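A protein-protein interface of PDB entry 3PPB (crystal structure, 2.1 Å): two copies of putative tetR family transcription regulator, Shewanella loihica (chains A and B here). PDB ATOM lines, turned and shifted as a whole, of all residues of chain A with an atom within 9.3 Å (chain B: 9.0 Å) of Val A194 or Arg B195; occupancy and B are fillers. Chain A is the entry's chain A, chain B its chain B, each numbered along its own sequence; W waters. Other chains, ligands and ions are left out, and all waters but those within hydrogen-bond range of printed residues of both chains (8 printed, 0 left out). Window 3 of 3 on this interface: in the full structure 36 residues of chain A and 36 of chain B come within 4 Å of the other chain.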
ATOM      1  N   LYS A  83     -33.776  29.852 -25.761  1.00  0.00           N
ATOM      2  CA  LYS A  83     -34.043  28.450 -25.455  1.00  0.00           C
ATOM      3  C   LYS A  83     -35.133  27.904 -26.378  1.00  0.00           C
ATOM      4  O   LYS A  83     -35.010  26.785 -26.880  1.00  0.00           O
ATOM      5  CB  LYS A  83     -34.417  28.275 -23.981  1.00  0.00           C
ATOM      6  CG  LYS A  83     -34.499  26.804 -23.557  1.00  0.00           C
ATOM      7  CD  LYS A  83     -34.981  26.675 -22.146  1.00  0.00           C
ATOM      8  CE  LYS A  83     -34.898  25.238 -21.699  1.00  0.00           C
ATOM      9  NZ  LYS A  83     -34.994  25.152 -20.222  1.00  0.00           N
ATOM     10  N   ILE A 136     -24.767  30.650 -29.744  1.00  0.00           N
ATOM     11  CA  ILE A 136     -24.058  30.334 -28.496  1.00  0.00           C
ATOM     12  C   ILE A 136     -23.546  31.649 -27.862  1.00  0.00           C
ATOM     13  O   ILE A 136     -23.754  31.842 -26.658  1.00  0.00           O
ATOM     14  CB  ILE A 136     -22.920  29.294 -28.680  1.00  0.00           C
ATOM     15  CG1 ILE A 136     -23.465  27.953 -29.231  1.00  0.00           C
ATOM     16  CG2 ILE A 136     -22.141  29.100 -27.372  1.00  0.00           C
ATOM     17  CD1 ILE A 136     -22.362  27.028 -29.845  1.00  0.00           C
ATOM     18  N   GLY A 139     -26.372  33.459 -26.251  1.00  0.00           N
ATOM     19  CA  GLY A 139     -26.745  32.762 -25.023  1.00  0.00           C
ATOM     20  C   GLY A 139     -25.772  32.979 -23.889  1.00  0.00           C
ATOM     21  O   GLY A 139     -26.171  32.968 -22.723  1.00  0.00           O
ATOM     22  N   GLN A 140     -24.484  33.167 -24.223  1.00  0.00           N
ATOM     23  CA  GLN A 140     -23.453  33.413 -23.225  1.00  0.00           C
ATOM     24  C   GLN A 140     -23.609  34.839 -22.689  1.00  0.00           C
ATOM     25  O   GLN A 140     -23.507  35.047 -21.481  1.00  0.00           O
ATOM     26  CB  GLN A 140     -22.050  33.178 -23.818  1.00  0.00           C
ATOM     27  CG  GLN A 140     -21.728  31.702 -24.001  1.00  0.00           C
ATOM     28  CD  GLN A 140     -20.392  31.440 -24.682  1.00  0.00           C
ATOM     29  OE1 GLN A 140     -19.882  32.256 -25.465  1.00  0.00           O
ATOM     30  NE2 GLN A 140     -19.804  30.274 -24.418  1.00  0.00           N
ATOM     31  N   ALA A 141     -23.884  35.807 -23.595  1.00  0.00           N
ATOM     32  CA  ALA A 141     -24.070  37.224 -23.269  1.00  0.00           C
ATOM     33  C   ALA A 141     -25.316  37.442 -22.410  1.00  0.00           C
ATOM     34  O   ALA A 141     -25.301  38.330 -21.573  1.00  0.00           O
ATOM     35  CB  ALA A 141     -24.169  38.047 -24.545  1.00  0.00           C
ATOM     36  N   SER A 142     -26.375  36.629 -22.591  1.00  0.00           N
ATOM     37  CA  SER A 142     -27.630  36.755 -21.833  1.00  0.00           C
ATOM     38  C   SER A 142     -27.583  36.005 -20.486  1.00  0.00           C
ATOM     39  O   SER A 142     -28.540  36.077 -19.709  1.00  0.00           O
ATOM     40  CB  SER A 142     -28.805  36.247 -22.661  1.00  0.00           C
ATOM     41  OG  SER A 142     -28.716  34.847 -22.850  1.00  0.00           O
ATOM     42  N   GLY A 143     -26.488  35.288 -20.237  1.00  0.00           N
ATOM     43  CA  GLY A 143     -26.306  34.517 -19.017  1.00  0.00           C
ATOM     44  C   GLY A 143     -27.048  33.200 -18.982  1.00  0.00           C
ATOM     45  O   GLY A 143     -27.224  32.642 -17.902  1.00  0.00           O
ATOM     46  N   GLU A 144     -27.500  32.686 -20.151  1.00  0.00           N
ATOM     47  CA  GLU A 144     -28.181  31.398 -20.229  1.00  0.00           C
ATOM     48  C   GLU A 144     -27.201  30.252 -20.479  1.00  0.00           C
ATOM     49  O   GLU A 144     -27.449  29.157 -20.007  1.00  0.00           O
ATOM     50  CB  GLU A 144     -29.230  31.381 -21.360  1.00  0.00           C
ATOM     51  CG  GLU A 144     -30.465  32.214 -21.087  1.00  0.00           C
ATOM     52  CD  GLU A 144     -31.356  32.332 -22.304  1.00  0.00           C
ATOM     53  OE1 GLU A 144     -31.102  33.234 -23.137  1.00  0.00           O
ATOM     54  OE2 GLU A 144     -32.280  31.497 -22.447  1.00  0.00           O
ATOM     55  N   LEU A 145     -26.117  30.494 -21.254  1.00  0.00           N
ATOM     56  CA  LEU A 145     -25.162  29.444 -21.622  1.00  0.00           C
ATOM     57  C   LEU A 145     -23.809  29.629 -20.952  1.00  0.00           C
ATOM     58  O   LEU A 145     -23.351  30.752 -20.764  1.00  0.00           O
ATOM     59  CB  LEU A 145     -24.986  29.366 -23.164  1.00  0.00           C
ATOM     60  CG  LEU A 145     -26.270  29.154 -23.984  1.00  0.00           C
ATOM     61  CD1 LEU A 145     -25.973  29.073 -25.478  1.00  0.00           C
ATOM     62  CD2 LEU A 145     -27.062  27.940 -23.491  1.00  0.00           C
ATOM     63  N   ALA A 146     -23.190  28.511 -20.573  1.00  0.00           N
ATOM     64  CA  ALA A 146     -21.874  28.466 -19.944  1.00  0.00           C
ATOM     65  C   ALA A 146     -20.801  29.000 -20.894  1.00  0.00           C
ATOM     66  O   ALA A 146     -20.956  28.974 -22.133  1.00  0.00           O
ATOM     67  CB  ALA A 146     -21.545  27.039 -19.539  1.00  0.00           C
ATOM     68  N   GLU A 147     -19.709  29.488 -20.309  1.00  0.00           N
ATOM     69  CA  GLU A 147     -18.626  30.076 -21.080  1.00  0.00           C
ATOM     70  C   GLU A 147     -17.490  29.095 -21.283  1.00  0.00           C
ATOM     71  O   GLU A 147     -16.446  29.209 -20.641  1.00  0.00           O
ATOM     72  CB  GLU A 147     -18.121  31.363 -20.418  1.00  0.00           C
ATOM     73  CG  GLU A 147     -19.202  32.414 -20.361  1.00  0.00           C
ATOM     74  CD  GLU A 147     -18.846  33.581 -19.499  1.00  0.00           C
ATOM     75  OE1 GLU A 147     -19.187  33.540 -18.300  1.00  0.00           O
ATOM     76  OE2 GLU A 147     -18.241  34.537 -20.025  1.00  0.00           O
ATOM     77  N   TYR A 148     -17.693  28.142 -22.192  1.00  0.00           N
ATOM     78  CA  TYR A 148     -16.630  27.191 -22.556  1.00  0.00           C
ATOM     79  C   TYR A 148     -16.058  27.639 -23.900  1.00  0.00           C
ATOM     80  O   TYR A 148     -16.736  28.448 -24.537  1.00  0.00           O
ATOM     81  CB  TYR A 148     -17.177  25.754 -22.631  1.00  0.00           C
ATOM     82  CG  TYR A 148     -18.026  25.314 -21.452  1.00  0.00           C
ATOM     83  CD1 TYR A 148     -17.567  25.448 -20.142  1.00  0.00           C
ATOM     84  CD2 TYR A 148     -19.262  24.707 -21.649  1.00  0.00           C
ATOM     85  CE1 TYR A 148     -18.344  25.041 -19.054  1.00  0.00           C
ATOM     86  CE2 TYR A 148     -20.029  24.258 -20.573  1.00  0.00           C
ATOM     87  CZ  TYR A 148     -19.571  24.438 -19.275  1.00  0.00           C
ATOM     88  OH  TYR A 148     -20.347  24.042 -18.211  1.00  0.00           O
ATOM     89  N   MET A 153     -17.807  23.870 -27.879  1.00  0.00           N
ATOM     90  CA  MET A 153     -19.260  23.857 -27.731  1.00  0.00           C
ATOM     91  C   MET A 153     -19.926  23.503 -29.075  1.00  0.00           C
ATOM     92  O   MET A 153     -20.870  22.732 -29.064  1.00  0.00           O
ATOM     93  CB  MET A 153     -19.750  25.204 -27.177  1.00  0.00           C
ATOM     94  CG  MET A 153     -19.218  25.485 -25.753  1.00  0.00           C
ATOM     95  SD  MET A 153     -19.934  27.142 -25.082  1.00  0.00           S
ATOM     96  CE  MET A 153     -21.655  26.541 -24.522  1.00  0.00           C
ATOM     97  N   ALA A 186     -33.246  17.961 -23.705  1.00  0.00           N
ATOM     98  CA  ALA A 186     -32.735  18.198 -22.350  1.00  0.00           C
ATOM     99  C   ALA A 186     -31.231  17.905 -22.280  1.00  0.00           C
ATOM    100  O   ALA A 186     -30.480  18.735 -21.759  1.00  0.00           O
ATOM    101  CB  ALA A 186     -33.501  17.360 -21.334  1.00  0.00           C
ATOM    102  N   LEU A 187     -30.775  16.779 -22.891  1.00  0.00           N
ATOM    103  CA  LEU A 187     -29.345  16.422 -22.913  1.00  0.00           C
ATOM    104  C   LEU A 187     -28.580  17.479 -23.682  1.00  0.00           C
ATOM    105  O   LEU A 187     -27.525  17.888 -23.238  1.00  0.00           O
ATOM    106  CB  LEU A 187     -29.099  15.031 -23.520  1.00  0.00           C
ATOM    107  CG  LEU A 187     -29.487  13.828 -22.631  1.00  0.00           C
ATOM    108  CD1 LEU A 187     -29.849  12.639 -23.469  1.00  0.00           C
ATOM    109  CD2 LEU A 187     -28.391  13.464 -21.611  1.00  0.00           C
ATOM    110  N   TRP A 189     -29.501  20.881 -24.394  1.00  0.00           N
ATOM    111  CA  TRP A 189     -29.533  22.158 -23.705  1.00  0.00           C
ATOM    112  C   TRP A 189     -28.700  22.140 -22.420  1.00  0.00           C
ATOM    113  O   TRP A 189     -27.904  23.061 -22.206  1.00  0.00           O
ATOM    114  CB  TRP A 189     -30.989  22.570 -23.375  1.00  0.00           C
ATOM    115  CG  TRP A 189     -31.060  23.947 -22.771  1.00  0.00           C
ATOM    116  CD1 TRP A 189     -31.265  24.257 -21.456  1.00  0.00           C
ATOM    117  CD2 TRP A 189     -30.879  25.204 -23.458  1.00  0.00           C
ATOM    118  NE1 TRP A 189     -31.233  25.627 -21.282  1.00  0.00           N
ATOM    119  CE2 TRP A 189     -30.991  26.230 -22.494  1.00  0.00           C
ATOM    120  CE3 TRP A 189     -30.632  25.561 -24.805  1.00  0.00           C
ATOM    121  CZ2 TRP A 189     -30.872  27.596 -22.829  1.00  0.00           C
ATOM    122  CZ3 TRP A 189     -30.530  26.911 -25.133  1.00  0.00           C
ATOM    123  CH2 TRP A 189     -30.665  27.911 -24.153  1.00  0.00           C
ATOM    124  N   ASN A 190     -28.877  21.105 -21.567  1.00  0.00           N
ATOM    125  CA  ASN A 190     -28.203  21.028 -20.264  1.00  0.00           C
ATOM    126  C   ASN A 190     -26.690  20.896 -20.377  1.00  0.00           C
ATOM    127  O   ASN A 190     -25.985  21.302 -19.448  1.00  0.00           O
ATOM    128  CB  ASN A 190     -28.795  19.930 -19.398  1.00  0.00           C
ATOM    129  CG  ASN A 190     -30.176  20.297 -18.932  1.00  0.00           C
ATOM    130  OD1 ASN A 190     -30.607  21.445 -19.043  1.00  0.00           O
ATOM    131  ND2 ASN A 190     -30.919  19.329 -18.438  1.00  0.00           N
ATOM    132  N   ALA A 191     -26.176  20.384 -21.504  1.00  0.00           N
ATOM    133  CA  ALA A 191     -24.717  20.346 -21.683  1.00  0.00           C
ATOM    134  C   ALA A 191     -24.155  21.759 -21.699  1.00  0.00           C
ATOM    135  O   ALA A 191     -23.119  22.000 -21.098  1.00  0.00           O
ATOM    136  CB  ALA A 191     -24.347  19.639 -23.001  1.00  0.00           C
ATOM    137  N   MET A 192     -24.871  22.690 -22.355  1.00  0.00           N
ATOM    138  CA  MET A 192     -24.491  24.095 -22.582  1.00  0.00           C
ATOM    139  C   MET A 192     -24.914  25.080 -21.513  1.00  0.00           C
ATOM    140  O   MET A 192     -24.292  26.127 -21.384  1.00  0.00           O
ATOM    141  CB  MET A 192     -25.167  24.607 -23.868  1.00  0.00           C
ATOM    142  CG  MET A 192     -24.842  23.846 -25.131  1.00  0.00           C
ATOM    143  SD  MET A 192     -25.433  24.918 -26.631  1.00  0.00           S
ATOM    144  CE  MET A 192     -27.376  24.681 -26.482  1.00  0.00           C
ATOM    145  N   ALA A 193     -26.084  24.850 -20.867  1.00  0.00           N
ATOM    146  CA  ALA A 193     -26.662  25.824 -19.944  1.00  0.00           C
ATOM    147  C   ALA A 193     -25.767  26.090 -18.740  1.00  0.00           C
ATOM    148  O   ALA A 193     -25.070  25.174 -18.286  1.00  0.00           O
ATOM    149  CB  ALA A 193     -28.043  25.356 -19.480  1.00  0.00           C
ATOM    150  N   VAL A 194     -25.803  27.346 -18.210  1.00  0.00           N
ATOM    151  CA  VAL A 194     -25.055  27.756 -17.011  1.00  0.00           C
ATOM    152  C   VAL A 194     -25.558  26.962 -15.803  1.00  0.00           C
ATOM    153  O   VAL A 194     -26.767  26.693 -15.697  1.00  0.00           O
ATOM    154  CB  VAL A 194     -25.139  29.275 -16.672  1.00  0.00           C
ATOM    155  CG1 VAL A 194     -24.249  30.125 -17.554  1.00  0.00           C
ATOM    156  CG2 VAL A 194     -26.576  29.783 -16.676  1.00  0.00           C
ATOM    157  N   ARG A 195     -24.651  26.649 -14.873  1.00  0.00           N
ATOM    158  CA  ARG A 195     -24.958  25.969 -13.607  1.00  0.00           C
ATOM    159  C   ARG A 195     -24.370  26.767 -12.444  1.00  0.00           C
ATOM    160  O   ARG A 195     -23.326  27.426 -12.661  1.00  0.00           O
ATOM    161  CB  ARG A 195     -24.417  24.546 -13.614  1.00  0.00           C
ATOM    162  CG  ARG A 195     -25.339  23.592 -14.381  1.00  0.00           C
ATOM    163  CD  ARG A 195     -25.176  22.144 -13.958  1.00  0.00           C
ATOM    164  NE  ARG A 195     -25.650  21.913 -12.594  1.00  0.00           N
ATOM    165  CZ  ARG A 195     -26.637  21.084 -12.264  1.00  0.00           C
ATOM    166  NH1 ARG A 195     -27.248  20.359 -13.196  1.00  0.00           N
ATOM    167  NH2 ARG A 195     -27.016  20.968 -10.998  1.00  0.00           N
ATOM    168  OXT ARG A 195     -24.965  26.759 -11.337  1.00  0.00           O
ATOM    169  N   GLY B 143     -29.778  10.545  -6.982  1.00  0.00           N
ATOM    170  CA  GLY B 143     -30.296  11.880  -7.255  1.00  0.00           C
ATOM    171  C   GLY B 143     -29.293  12.841  -7.880  1.00  0.00           C
ATOM    172  O   GLY B 143     -29.487  14.057  -7.809  1.00  0.00           O
ATOM    173  N   GLU B 144     -28.232  12.310  -8.525  1.00  0.00           N
ATOM    174  CA  GLU B 144     -27.189  13.142  -9.142  1.00  0.00           C
ATOM    175  C   GLU B 144     -27.381  13.293 -10.635  1.00  0.00           C
ATOM    176  O   GLU B 144     -27.037  14.349 -11.161  1.00  0.00           O
ATOM    177  CB  GLU B 144     -25.781  12.588  -8.847  1.00  0.00           C
ATOM    178  CG  GLU B 144     -25.426  12.774  -7.376  1.00  0.00           C
ATOM    179  CD  GLU B 144     -24.259  11.975  -6.838  1.00  0.00           C
ATOM    180  OE1 GLU B 144     -24.273  10.727  -6.931  1.00  0.00           O
ATOM    181  OE2 GLU B 144     -23.370  12.603  -6.230  1.00  0.00           O
ATOM    182  N   LEU B 145     -27.976  12.270 -11.306  1.00  0.00           N
ATOM    183  CA  LEU B 145     -28.214  12.274 -12.751  1.00  0.00           C
ATOM    184  C   LEU B 145     -29.704  12.317 -13.081  1.00  0.00           C
ATOM    185  O   LEU B 145     -30.534  11.739 -12.365  1.00  0.00           O
ATOM    186  CB  LEU B 145     -27.562  11.071 -13.444  1.00  0.00           C
ATOM    187  CG  LEU B 145     -26.031  10.916 -13.218  1.00  0.00           C
ATOM    188  CD1 LEU B 145     -25.498   9.683 -13.967  1.00  0.00           C
ATOM    189  CD2 LEU B 145     -25.251  12.215 -13.592  1.00  0.00           C
ATOM    190  N   ALA B 146     -30.033  13.031 -14.170  1.00  0.00           N
ATOM    191  CA  ALA B 146     -31.400  13.181 -14.660  1.00  0.00           C
ATOM    192  C   ALA B 146     -31.986  11.834 -15.080  1.00  0.00           C
ATOM    193  O   ALA B 146     -31.236  10.904 -15.436  1.00  0.00           O
ATOM    194  CB  ALA B 146     -31.419  14.139 -15.830  1.00  0.00           C
ATOM    195  N   GLU B 147     -33.336  11.731 -15.052  1.00  0.00           N
ATOM    196  CA  GLU B 147     -33.988  10.489 -15.403  1.00  0.00           C
ATOM    197  C   GLU B 147     -34.493  10.501 -16.849  1.00  0.00           C
ATOM    198  O   GLU B 147     -35.687  10.627 -17.104  1.00  0.00           O
ATOM    199  CB  GLU B 147     -35.114  10.151 -14.425  1.00  0.00           C
ATOM    200  CG  GLU B 147     -34.618  10.058 -12.991  1.00  0.00           C
ATOM    201  CD  GLU B 147     -35.749   9.948 -12.000  1.00  0.00           C
ATOM    202  OE1 GLU B 147     -36.314  10.996 -11.607  1.00  0.00           O
ATOM    203  OE2 GLU B 147     -36.135   8.803 -11.679  1.00  0.00           O
ATOM    204  N   TYR B 148     -33.569  10.336 -17.790  1.00  0.00           N
ATOM    205  CA  TYR B 148     -33.881  10.214 -19.208  1.00  0.00           C
ATOM    206  C   TYR B 148     -33.723   8.735 -19.567  1.00  0.00           C
ATOM    207  O   TYR B 148     -33.071   8.045 -18.783  1.00  0.00           O
ATOM    208  CB  TYR B 148     -32.927  11.083 -20.069  1.00  0.00           C
ATOM    209  CG  TYR B 148     -32.713  12.501 -19.609  1.00  0.00           C
ATOM    210  CD1 TYR B 148     -33.789  13.335 -19.327  1.00  0.00           C
ATOM    211  CD2 TYR B 148     -31.431  13.034 -19.517  1.00  0.00           C
ATOM    212  CE1 TYR B 148     -33.592  14.649 -18.886  1.00  0.00           C
ATOM    213  CE2 TYR B 148     -31.223  14.360 -19.142  1.00  0.00           C
ATOM    214  CZ  TYR B 148     -32.307  15.162 -18.818  1.00  0.00           C
ATOM    215  OH  TYR B 148     -32.091  16.458 -18.393  1.00  0.00           O
ATOM    216  N   TRP B 189     -20.642  16.106 -18.206  1.00  0.00           N
ATOM    217  CA  TRP B 189     -21.370  15.960 -16.944  1.00  0.00           C
ATOM    218  C   TRP B 189     -22.699  16.720 -16.939  1.00  0.00           C
ATOM    219  O   TRP B 189     -23.716  16.149 -16.552  1.00  0.00           O
ATOM    220  CB  TRP B 189     -20.504  16.442 -15.745  1.00  0.00           C
ATOM    221  CG  TRP B 189     -21.177  16.208 -14.424  1.00  0.00           C
ATOM    222  CD1 TRP B 189     -21.786  17.141 -13.636  1.00  0.00           C
ATOM    223  CD2 TRP B 189     -21.355  14.946 -13.770  1.00  0.00           C
ATOM    224  NE1 TRP B 189     -22.328  16.535 -12.518  1.00  0.00           N
ATOM    225  CE2 TRP B 189     -22.090  15.186 -12.584  1.00  0.00           C
ATOM    226  CE3 TRP B 189     -20.986  13.618 -14.088  1.00  0.00           C
ATOM    227  CZ2 TRP B 189     -22.437  14.155 -11.693  1.00  0.00           C
ATOM    228  CZ3 TRP B 189     -21.334  12.600 -13.209  1.00  0.00           C
ATOM    229  CH2 TRP B 189     -22.049  12.871 -12.030  1.00  0.00           C
ATOM    230  N   ASN B 190     -22.695  18.000 -17.356  1.00  0.00           N
ATOM    231  CA  ASN B 190     -23.900  18.844 -17.312  1.00  0.00           C
ATOM    232  C   ASN B 190     -25.001  18.362 -18.232  1.00  0.00           C
ATOM    233  O   ASN B 190     -26.175  18.643 -17.954  1.00  0.00           O
ATOM    234  CB  ASN B 190     -23.560  20.297 -17.589  1.00  0.00           C
ATOM    235  CG  ASN B 190     -22.803  20.898 -16.413  1.00  0.00           C
ATOM    236  OD1 ASN B 190     -22.749  20.321 -15.326  1.00  0.00           O
ATOM    237  ND2 ASN B 190     -22.178  22.036 -16.605  1.00  0.00           N
ATOM    238  N   ALA B 191     -24.657  17.612 -19.312  1.00  0.00           N
ATOM    239  CA  ALA B 191     -25.716  17.028 -20.154  1.00  0.00           C
ATOM    240  C   ALA B 191     -26.568  16.069 -19.330  1.00  0.00           C
ATOM    241  O   ALA B 191     -27.782  16.102 -19.450  1.00  0.00           O
ATOM    242  CB  ALA B 191     -25.106  16.285 -21.341  1.00  0.00           C
ATOM    243  N   MET B 192     -25.936  15.271 -18.472  1.00  0.00           N
ATOM    244  CA  MET B 192     -26.537  14.210 -17.629  1.00  0.00           C
ATOM    245  C   MET B 192     -27.079  14.633 -16.281  1.00  0.00           C
ATOM    246  O   MET B 192     -27.973  13.966 -15.763  1.00  0.00           O
ATOM    247  CB  MET B 192     -25.465  13.148 -17.298  1.00  0.00           C
ATOM    248  CG  MET B 192     -24.844  12.472 -18.502  1.00  0.00           C
ATOM    249  SD  MET B 192     -23.911  10.875 -17.915  1.00  0.00           S
ATOM    250  CE  MET B 192     -22.375  11.740 -17.022  1.00  0.00           C
ATOM    251  N   ALA B 193     -26.416  15.624 -15.622  1.00  0.00           N
ATOM    252  CA  ALA B 193     -26.743  16.002 -14.244  1.00  0.00           C
ATOM    253  C   ALA B 193     -28.164  16.518 -14.091  1.00  0.00           C
ATOM    254  O   ALA B 193     -28.672  17.156 -15.000  1.00  0.00           O
ATOM    255  CB  ALA B 193     -25.760  17.050 -13.743  1.00  0.00           C
ATOM    256  N   VAL B 194     -28.782  16.269 -12.903  1.00  0.00           N
ATOM    257  CA  VAL B 194     -30.133  16.744 -12.535  1.00  0.00           C
ATOM    258  C   VAL B 194     -30.175  18.249 -12.500  1.00  0.00           C
ATOM    259  O   VAL B 194     -29.200  18.882 -12.058  1.00  0.00           O
ATOM    260  CB  VAL B 194     -30.668  16.220 -11.167  1.00  0.00           C
ATOM    261  CG1 VAL B 194     -31.238  14.817 -11.260  1.00  0.00           C
ATOM    262  CG2 VAL B 194     -29.659  16.364 -10.040  1.00  0.00           C
ATOM    263  N   ARG B 195     -31.341  18.811 -12.913  1.00  0.00           N
ATOM    264  CA  ARG B 195     -31.610  20.252 -12.892  1.00  0.00           C
ATOM    265  C   ARG B 195     -32.919  20.531 -12.153  1.00  0.00           C
ATOM    266  O   ARG B 195     -33.782  19.629 -12.128  1.00  0.00           O
ATOM    267  CB  ARG B 195     -31.621  20.846 -14.304  1.00  0.00           C
ATOM    268  CG  ARG B 195     -30.192  21.072 -14.816  1.00  0.00           C
ATOM    269  CD  ARG B 195     -30.077  22.137 -15.870  1.00  0.00           C
ATOM    270  NE  ARG B 195     -30.305  23.468 -15.324  1.00  0.00           N
ATOM    271  CZ  ARG B 195     -29.442  24.466 -15.429  1.00  0.00           C
ATOM    272  NH1 ARG B 195     -28.291  24.292 -16.064  1.00  0.00           N
ATOM    273  NH2 ARG B 195     -29.723  25.651 -14.904  1.00  0.00           N
ATOM    274  OXT ARG B 195     -33.040  21.605 -11.521  1.00  0.00           O
HETATM  275  O   HOH W   1     -22.848  19.984 -11.915  1.00  0.00           O
HETATM  276  O   HOH W   2     -33.356  17.861 -16.444  1.00  0.00           O
HETATM  277  O   HOH W   3     -22.883  23.364 -18.845  1.00  0.00           O
HETATM  278  O   HOH W   4     -26.525  22.474 -17.118  1.00  0.00           O
HETATM  279  O   HOH W   5     -21.002  24.895 -15.456  1.00  0.00           O
HETATM  280  O   HOH W   6     -27.407  19.467 -15.729  1.00  0.00           O
HETATM  281  O   HOH W   7     -27.119  18.587 -10.170  1.00  0.00           O
HETATM  282  O   HOH W   8     -29.646  16.985 -17.572  1.00  0.00           O
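Asn A190 touches its own counterpart, Asn B190. Ala B191 touches its own counterpart, Ala A191. Ala A193 touches Arg B195, and with the chains exchanged Arg A195 touches Ala B193. Val A194 touches Arg B195, and with the chains exchanged Arg A195 touches Val B194. Positions printed for both chains: 143, 144, 145, 146, 147, 148, 189, 190, 191, 192, 193, 194 and 195. Of the 16 pairs that touch across the chains among the printed residues, 13 have their exchanged pair printed and touching as well.
Water W7 bridges the guanidinium group (NH2) of Arg A195 (2.5 Å) and the backbone carbonyl oxygen (O) of Val B194 (2.8 Å). Water W8 lies within hydrogen-bond range of OH of Tyr B148 (2.6 Å), O of Ala B193 (2.8 Å), O of Ala B191 (2.8 Å) and ND2 of Asn A190 (2.8 Å). Water W3 lies within hydrogen-bond range of the backbone carbonyl oxygen (O) of Ala A191 (2.6 Å), the side-chain amide nitrogen (ND2) of Asn B190 (2.7 Å), the side-chain hydroxyl (OH) of Tyr A148 (2.7 Å) and the backbone carbonyl oxygen (O) of Ala A193 (2.9 Å). Water W4 lies within hydrogen-bond range of O of Asn A190 (2.7 Å), NH1 of Arg B195 (2.7 Å) and O of Ala A193 (3.3 Å). Water W5 bridges OH of Tyr A148 and ND2 of Asn B190. Water W1 bridges OD1 of Asn B190 (3.4 Å) and NE of Arg A195 (3.5 Å).
The side-chain amide nitrogen (ND2) of Asn B190 lies within hydrogen-bond range of the side-chain hydroxyl (OH) of Tyr A148 (3.2 Å). The side-chain amide nitrogen (ND2) of Asn A190 lies within hydrogen-bond range of the side-chain hydroxyl (OH) of Tyr B148, 3.1 Å away. O of Val A194 lies within hydrogen-bond range of NH1 of Arg B195 (2.9 Å). NH1 of Arg A195 is in hydrogen-bond range of O of Val B194, 2.7 Å away. The backbone carbonyl oxygen (O) of Asn B190 lies close to the backbone carbonyl oxygen (O) of Asn A190.
Of the 13 printed residues of chain B, 6 touch a printed residue of chain A. Hydrophobic or aromatic side chains of chain B within 4 Å of the printed part of chain A: Tyr B148, Ala B191 and Ala B193. Hydrophobic or aromatic side chains of chain A within 4 Å of the printed part of chain B: Tyr A148, Ala A186, Leu A187, Ala A191 and Ala A193. Among the printed residues, no Asp or Glu carboxylate lies within 4 Å of a Lys or Arg side-chain nitrogen of the other chain.
Of the printed residues of chain B, Tyr A148 touches Asn B190. Met A153 touches none of the printed residues of chain B. Printed residues of chain B within 4 Å of Leu A187: Tyr B148 (3.7 Å) and Ala B191 (3.5 Å). Ala A193 touches just one residue of chain B: Arg B195. Val A194 touches one residue of chain B. Of chain A, only Arg A195 comes within 4 Å of Val B194. Of chain A, only Asn A190 (3.3 Å), Ala A193 (3.6 Å), Val A194 (2.9 Å) and Arg A195 (3.4 Å) come within 4 Å of Arg B195. The nearest residue of chain B that does not touch Val A194 is Asn B190 (6.0 Å). The nearest residue of chain A that does not touch Arg B195 is Trp A189 (6.1 Å).
The backbone NH (N) of Val A194 lies within hydrogen-bond range of the backbone carbonyl oxygen (O) of Glu A144, at 3.0 Å. The backbone NH of Tyr A148 sits at hydrogen-bond distance from the side-chain sulfur of Met A153 (3.8 Å). The backbone carbonyl oxygen (O) of Ala A186 lies close to the side-chain amide nitrogen (ND2) of Asn A190, at 3.4 Å. N of Val B194 sits at hydrogen-bond distance from O of Glu B144 (3.1 Å).
Ala A186 touches Tyr B148 (CB to OH, 3.4 Å). Tyr B148 touches Leu A187 (CD2 to CD2, 3.7 Å). Asn A190 touches Ala B191. Asn A190 touches Arg B195. Ala A191 touches Asn B190 (O to CB, 3.9 Å). Ala A191 touches Ala B191 (CA to N, 3.6 Å). Ala A193 touches Arg B195. Asn B190 touches Arg A195 (OD1 to CD, 3.3 Å). Arg A195 touches Ala B193 (NH1 to CB, 3.7 Å). Arg A195 touches Arg B195 (NH1 to CG, 3.4 Å).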
